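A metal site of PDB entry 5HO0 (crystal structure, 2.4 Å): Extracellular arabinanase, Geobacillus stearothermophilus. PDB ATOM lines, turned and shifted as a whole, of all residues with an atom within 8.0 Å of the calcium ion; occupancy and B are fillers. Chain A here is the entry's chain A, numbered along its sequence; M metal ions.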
ATOM      1  N   HIS A 647      21.539 -23.327  -7.819  1.00  0.00           N
ATOM      2  CA  HIS A 647      20.204 -23.855  -7.502  1.00  0.00           C
ATOM      3  C   HIS A 647      19.422 -24.268  -8.739  1.00  0.00           C
ATOM      4  O   HIS A 647      18.997 -23.424  -9.546  1.00  0.00           O
ATOM      5  CB  HIS A 647      19.409 -22.830  -6.706  1.00  0.00           C
ATOM      6  CG  HIS A 647      18.143 -23.387  -6.128  1.00  0.00           C
ATOM      7  ND1 HIS A 647      17.076 -22.590  -5.753  1.00  0.00           N
ATOM      8  CD2 HIS A 647      17.768 -24.659  -5.863  1.00  0.00           C
ATOM      9  CE1 HIS A 647      16.111 -23.351  -5.269  1.00  0.00           C
ATOM     10  NE2 HIS A 647      16.506 -24.611  -5.334  1.00  0.00           N
ATOM     11  N   TYR A 648      19.225 -25.574  -8.892  1.00  0.00           N
ATOM     12  CA  TYR A 648      18.408 -26.121  -9.963  1.00  0.00           C
ATOM     13  C   TYR A 648      17.138 -26.588  -9.309  1.00  0.00           C
ATOM     14  O   TYR A 648      17.079 -27.667  -8.700  1.00  0.00           O
ATOM     15  CB  TYR A 648      19.124 -27.225 -10.736  1.00  0.00           C
ATOM     16  CG  TYR A 648      20.381 -26.715 -11.393  1.00  0.00           C
ATOM     17  CD1 TYR A 648      21.581 -26.635 -10.689  1.00  0.00           C
ATOM     18  CD2 TYR A 648      20.380 -26.266 -12.699  1.00  0.00           C
ATOM     19  CE1 TYR A 648      22.752 -26.148 -11.278  1.00  0.00           C
ATOM     20  CE2 TYR A 648      21.537 -25.765 -13.289  1.00  0.00           C
ATOM     21  CZ  TYR A 648      22.725 -25.724 -12.566  1.00  0.00           C
ATOM     22  OH  TYR A 648      23.887 -25.246 -13.159  1.00  0.00           O
ATOM     23  N   SER A 649      16.129 -25.723  -9.405  1.00  0.00           N
ATOM     24  CA  SER A 649      14.800 -25.995  -8.926  1.00  0.00           C
ATOM     25  C   SER A 649      13.953 -26.675 -10.001  1.00  0.00           C
ATOM     26  O   SER A 649      13.033 -27.434  -9.653  1.00  0.00           O
ATOM     27  CB  SER A 649      14.139 -24.689  -8.555  1.00  0.00           C
ATOM     28  OG  SER A 649      14.332 -23.781  -9.615  1.00  0.00           O
ATOM     29  N   PHE A 650      14.275 -26.394 -11.276  1.00  0.00           N
ATOM     30  CA  PHE A 650      13.419 -26.760 -12.443  1.00  0.00           C
ATOM     31  C   PHE A 650      12.047 -26.061 -12.465  1.00  0.00           C
ATOM     32  O   PHE A 650      11.116 -26.549 -13.101  1.00  0.00           O
ATOM     33  CB  PHE A 650      13.224 -28.286 -12.518  1.00  0.00           C
ATOM     34  CG  PHE A 650      14.452 -29.052 -12.145  1.00  0.00           C
ATOM     35  CD1 PHE A 650      15.620 -28.922 -12.922  1.00  0.00           C
ATOM     36  CD2 PHE A 650      14.480 -29.838 -11.000  1.00  0.00           C
ATOM     37  CE1 PHE A 650      16.763 -29.575 -12.560  1.00  0.00           C
ATOM     38  CE2 PHE A 650      15.627 -30.501 -10.646  1.00  0.00           C
ATOM     39  CZ  PHE A 650      16.766 -30.373 -11.424  1.00  0.00           C
ATOM     40  N   ASP A 651      11.949 -24.931 -11.772  1.00  0.00           N
ATOM     41  CA  ASP A 651      10.648 -24.275 -11.528  1.00  0.00           C
ATOM     42  C   ASP A 651      10.211 -23.381 -12.689  1.00  0.00           C
ATOM     43  O   ASP A 651       9.050 -23.002 -12.741  1.00  0.00           O
ATOM     44  CB  ASP A 651      10.691 -23.436 -10.228  1.00  0.00           C
ATOM     45  CG  ASP A 651      10.506 -24.289  -8.992  1.00  0.00           C
ATOM     46  OD1 ASP A 651      10.513 -25.538  -9.106  1.00  0.00           O
ATOM     47  OD2 ASP A 651      10.373 -23.728  -7.885  1.00  0.00           O
ATOM     48  N   ASN A 652      11.157 -23.074 -13.585  1.00  0.00           N
ATOM     49  CA  ASN A 652      10.909 -22.263 -14.789  1.00  0.00           C
ATOM     50  C   ASN A 652      11.059 -23.059 -16.085  1.00  0.00           C
ATOM     51  O   ASN A 652      11.591 -22.558 -17.086  1.00  0.00           O
ATOM     52  CB  ASN A 652      11.805 -21.016 -14.805  1.00  0.00           C
ATOM     53  CG  ASN A 652      11.662 -20.202 -13.541  1.00  0.00           C
ATOM     54  OD1 ASN A 652      10.613 -20.236 -12.884  1.00  0.00           O
ATOM     55  ND2 ASN A 652      12.725 -19.476 -13.166  1.00  0.00           N
ATOM     56  N   TYR A 681       9.163 -32.237 -16.927  1.00  0.00           N
ATOM     57  CA  TYR A 681       8.950 -31.593 -15.640  1.00  0.00           C
ATOM     58  C   TYR A 681       7.587 -32.050 -15.198  1.00  0.00           C
ATOM     59  O   TYR A 681       6.658 -32.062 -15.998  1.00  0.00           O
ATOM     60  CB  TYR A 681       9.023 -30.086 -15.768  1.00  0.00           C
ATOM     61  CG  TYR A 681      10.308 -29.615 -16.395  1.00  0.00           C
ATOM     62  CD1 TYR A 681      11.457 -29.450 -15.622  1.00  0.00           C
ATOM     63  CD2 TYR A 681      10.384 -29.352 -17.759  1.00  0.00           C
ATOM     64  CE1 TYR A 681      12.649 -29.026 -16.202  1.00  0.00           C
ATOM     65  CE2 TYR A 681      11.581 -28.939 -18.347  1.00  0.00           C
ATOM     66  CZ  TYR A 681      12.706 -28.769 -17.558  1.00  0.00           C
ATOM     67  OH  TYR A 681      13.883 -28.362 -18.137  1.00  0.00           O
ATOM     68  N   ALA A 682       7.468 -32.515 -13.952  1.00  0.00           N
ATOM     69  CA  ALA A 682       6.180 -32.970 -13.420  1.00  0.00           C
ATOM     70  C   ALA A 682       6.064 -32.500 -11.989  1.00  0.00           C
ATOM     71  O   ALA A 682       7.042 -32.001 -11.427  1.00  0.00           O
ATOM     72  CB  ALA A 682       6.075 -34.476 -13.496  1.00  0.00           C
ATOM     73  N   ASP A 683       4.882 -32.666 -11.395  1.00  0.00           N
ATOM     74  CA  ASP A 683       4.581 -32.067 -10.075  1.00  0.00           C
ATOM     75  C   ASP A 683       5.493 -32.617  -8.960  1.00  0.00           C
ATOM     76  O   ASP A 683       5.600 -33.831  -8.770  1.00  0.00           O
ATOM     77  CB  ASP A 683       3.086 -32.205  -9.693  1.00  0.00           C
ATOM     78  CG  ASP A 683       2.287 -30.884  -9.860  1.00  0.00           C
ATOM     79  OD1 ASP A 683       2.673 -30.007 -10.660  1.00  0.00           O
ATOM     80  OD2 ASP A 683       1.247 -30.734  -9.181  1.00  0.00           O
ATOM     81  N   GLY A 684       6.125 -31.693  -8.238  1.00  0.00           N
ATOM     82  CA  GLY A 684       7.175 -32.016  -7.280  1.00  0.00           C
ATOM     83  C   GLY A 684       7.149 -31.222  -5.986  1.00  0.00           C
ATOM     84  O   GLY A 684       6.197 -30.461  -5.719  1.00  0.00           O
ATOM     85  N   LYS A 685       8.246 -31.385  -5.208  1.00  0.00           N
ATOM     86  CA  LYS A 685       8.334 -30.981  -3.798  1.00  0.00           C
ATOM     87  C   LYS A 685       8.181 -29.481  -3.566  1.00  0.00           C
ATOM     88  O   LYS A 685       7.457 -29.064  -2.664  1.00  0.00           O
ATOM     89  CB  LYS A 685       9.658 -31.461  -3.180  1.00  0.00           C
ATOM     90  CG  LYS A 685       9.631 -31.555  -1.665  1.00  0.00           C
ATOM     91  CD  LYS A 685       8.436 -32.367  -1.182  1.00  0.00           C
ATOM     92  CE  LYS A 685       8.712 -33.111   0.110  1.00  0.00           C
ATOM     93  NZ  LYS A 685       8.740 -32.215   1.289  1.00  0.00           N
ATOM     94  N   ILE A 686       8.892 -28.681  -4.340  1.00  0.00           N
ATOM     95  CA  ILE A 686       8.584 -27.267  -4.476  1.00  0.00           C
ATOM     96  C   ILE A 686       8.661 -26.961  -5.981  1.00  0.00           C
ATOM     97  O   ILE A 686       9.639 -27.306  -6.663  1.00  0.00           O
ATOM     98  CB  ILE A 686       9.409 -26.306  -3.534  1.00  0.00           C
ATOM     99  CG1 ILE A 686      10.473 -25.485  -4.285  1.00  0.00           C
ATOM    100  CG2 ILE A 686       9.990 -27.015  -2.312  1.00  0.00           C
ATOM    101  CD1 ILE A 686       9.917 -24.224  -4.924  1.00  0.00           C
ATOM    102  N   GLY A 687       7.586 -26.354  -6.489  1.00  0.00           N
ATOM    103  CA  GLY A 687       7.381 -26.131  -7.911  1.00  0.00           C
ATOM    104  C   GLY A 687       7.362 -27.434  -8.679  1.00  0.00           C
ATOM    105  O   GLY A 687       6.901 -28.480  -8.179  1.00  0.00           O
ATOM    106  N   LYS A 688       7.854 -27.347  -9.912  1.00  0.00           N
ATOM    107  CA  LYS A 688       8.081 -28.508 -10.776  1.00  0.00           C
ATOM    108  C   LYS A 688       9.446 -29.152 -10.461  1.00  0.00           C
ATOM    109  O   LYS A 688      10.468 -28.459 -10.396  1.00  0.00           O
ATOM    110  CB  LYS A 688       8.019 -28.100 -12.272  1.00  0.00           C
ATOM    111  CG  LYS A 688       6.812 -28.657 -13.045  1.00  0.00           C
ATOM    112  CD  LYS A 688       5.643 -27.686 -13.160  1.00  0.00           C
ATOM    113  CE  LYS A 688       4.321 -28.314 -12.694  1.00  0.00           C
ATOM    114  NZ  LYS A 688       3.855 -29.578 -13.335  1.00  0.00           N
ATOM    115  N   ALA A 689       9.439 -30.480 -10.235  1.00  0.00           N
ATOM    116  CA  ALA A 689      10.655 -31.309 -10.192  1.00  0.00           C
ATOM    117  C   ALA A 689      11.110 -31.727 -11.598  1.00  0.00           C
ATOM    118  O   ALA A 689      10.368 -31.564 -12.581  1.00  0.00           O
ATOM    119  CB  ALA A 689      10.409 -32.556  -9.347  1.00  0.00           C
ATOM    120  N   ALA A 690      12.327 -32.252 -11.692  1.00  0.00           N
ATOM    121  CA  ALA A 690      12.812 -32.841 -12.958  1.00  0.00           C
ATOM    122  C   ALA A 690      12.465 -34.314 -12.954  1.00  0.00           C
ATOM    123  O   ALA A 690      12.642 -34.988 -11.932  1.00  0.00           O
ATOM    124  CB  ALA A 690      14.312 -32.647 -13.141  1.00  0.00           C
ATOM    125  N   TRP A 772       9.173 -39.046  -1.686  1.00  0.00           N
ATOM    126  CA  TRP A 772      10.245 -38.054  -1.467  1.00  0.00           C
ATOM    127  C   TRP A 772      11.101 -38.359  -0.225  1.00  0.00           C
ATOM    128  O   TRP A 772      10.592 -38.757   0.840  1.00  0.00           O
ATOM    129  CB  TRP A 772       9.689 -36.638  -1.352  1.00  0.00           C
ATOM    130  CG  TRP A 772       9.076 -36.096  -2.607  1.00  0.00           C
ATOM    131  CD1 TRP A 772       7.745 -35.914  -2.843  1.00  0.00           C
ATOM    132  CD2 TRP A 772       9.764 -35.684  -3.797  1.00  0.00           C
ATOM    133  NE1 TRP A 772       7.562 -35.389  -4.105  1.00  0.00           N
ATOM    134  CE2 TRP A 772       8.783 -35.242  -4.713  1.00  0.00           C
ATOM    135  CE3 TRP A 772      11.109 -35.631  -4.179  1.00  0.00           C
ATOM    136  CZ2 TRP A 772       9.104 -34.761  -6.003  1.00  0.00           C
ATOM    137  CZ3 TRP A 772      11.427 -35.135  -5.452  1.00  0.00           C
ATOM    138  CH2 TRP A 772      10.428 -34.725  -6.349  1.00  0.00           C
ATOM    139  N   ILE A 825      13.925 -35.946  -9.210  1.00  0.00           N
ATOM    140  CA  ILE A 825      14.740 -35.280  -8.221  1.00  0.00           C
ATOM    141  C   ILE A 825      14.358 -33.770  -8.241  1.00  0.00           C
ATOM    142  O   ILE A 825      14.179 -33.162  -9.314  1.00  0.00           O
ATOM    143  CB  ILE A 825      16.257 -35.591  -8.413  1.00  0.00           C
ATOM    144  CG1 ILE A 825      16.792 -35.018  -9.714  1.00  0.00           C
ATOM    145  CG2 ILE A 825      16.502 -37.099  -8.411  1.00  0.00           C
ATOM    146  CD1 ILE A 825      17.404 -33.652  -9.527  1.00  0.00           C
ATOM    147  N   ASP A 826      14.175 -33.179  -7.053  1.00  0.00           N
ATOM    148  CA  ASP A 826      13.835 -31.772  -6.952  1.00  0.00           C
ATOM    149  C   ASP A 826      14.887 -30.986  -6.195  1.00  0.00           C
ATOM    150  O   ASP A 826      15.558 -31.507  -5.301  1.00  0.00           O
ATOM    151  CB  ASP A 826      12.447 -31.579  -6.289  1.00  0.00           C
ATOM    152  CG  ASP A 826      11.777 -30.251  -6.687  1.00  0.00           C
ATOM    153  OD1 ASP A 826      12.368 -29.528  -7.540  1.00  0.00           O
ATOM    154  OD2 ASP A 826      10.688 -29.936  -6.163  1.00  0.00           O
ATOM    155  N   GLU A 827      15.008 -29.717  -6.586  1.00  0.00           N
ATOM    156  CA  GLU A 827      15.683 -28.710  -5.776  1.00  0.00           C
ATOM    157  C   GLU A 827      17.103 -29.153  -5.459  1.00  0.00           C
ATOM    158  O   GLU A 827      17.409 -29.579  -4.330  1.00  0.00           O
ATOM    159  CB  GLU A 827      14.887 -28.442  -4.488  1.00  0.00           C
ATOM    160  CG  GLU A 827      13.519 -27.808  -4.731  1.00  0.00           C
ATOM    161  CD  GLU A 827      13.615 -26.521  -5.515  1.00  0.00           C
ATOM    162  OE1 GLU A 827      14.293 -25.586  -5.002  1.00  0.00           O
ATOM    163  OE2 GLU A 827      13.036 -26.435  -6.637  1.00  0.00           O
ATOM    164  N   LEU A 828      17.941 -29.089  -6.493  1.00  0.00           N
ATOM    165  CA  LEU A 828      19.334 -29.406  -6.354  1.00  0.00           C
ATOM    166  C   LEU A 828      20.051 -28.147  -5.896  1.00  0.00           C
ATOM    167  O   LEU A 828      20.204 -27.207  -6.677  1.00  0.00           O
ATOM    168  CB  LEU A 828      19.946 -29.882  -7.659  1.00  0.00           C
ATOM    169  CG  LEU A 828      21.463 -30.026  -7.528  1.00  0.00           C
ATOM    170  CD1 LEU A 828      21.801 -31.060  -6.437  1.00  0.00           C
ATOM    171  CD2 LEU A 828      22.122 -30.411  -8.839  1.00  0.00           C
HETATM  172 CA    CA M   1      11.394 -27.473  -8.060  1.00  0.00          CA
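Within 4 Å of the calcium ion: Ser 649, Asp 651, Ile 686, Lys 688, Asp 826 and Glu 827.
Along chain A the residues within 4 Å of the calcium ion span positions 649 to 827.
The calcium ion is bound by the backbone carbonyl oxygen (O) of Ile 686 (2.2 Å), the backbone carbonyl oxygen (O) of Ser 649 (2.3 Å), the side-chain carboxylate (OD1) of Asp 826 (2.3 Å), the side-chain carboxylate (OD1) of Asp 651 (2.4 Å), the side-chain carboxylate (OE2) of Glu 827 (2.4 Å) and the backbone carbonyl oxygen (O) of Lys 688 (2.7 Å).
The calcium ion has six donor atoms within binding distance.
The side-chain carboxylate of Asp 826 lies within hydrogen-bond range of the backbone NH of Lys 685, at 3.0 Å.
The side-chain carboxylate (OE1) of Glu 827 sits at hydrogen-bond distance from a ring nitrogen (NE2) of His 647 (2.4 Å).
The side-chain amino group (NZ) of Lys 688 is in salt-bridge range of the side-chain carboxylate (OD1) of Asp 683, at 3.0 Å.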
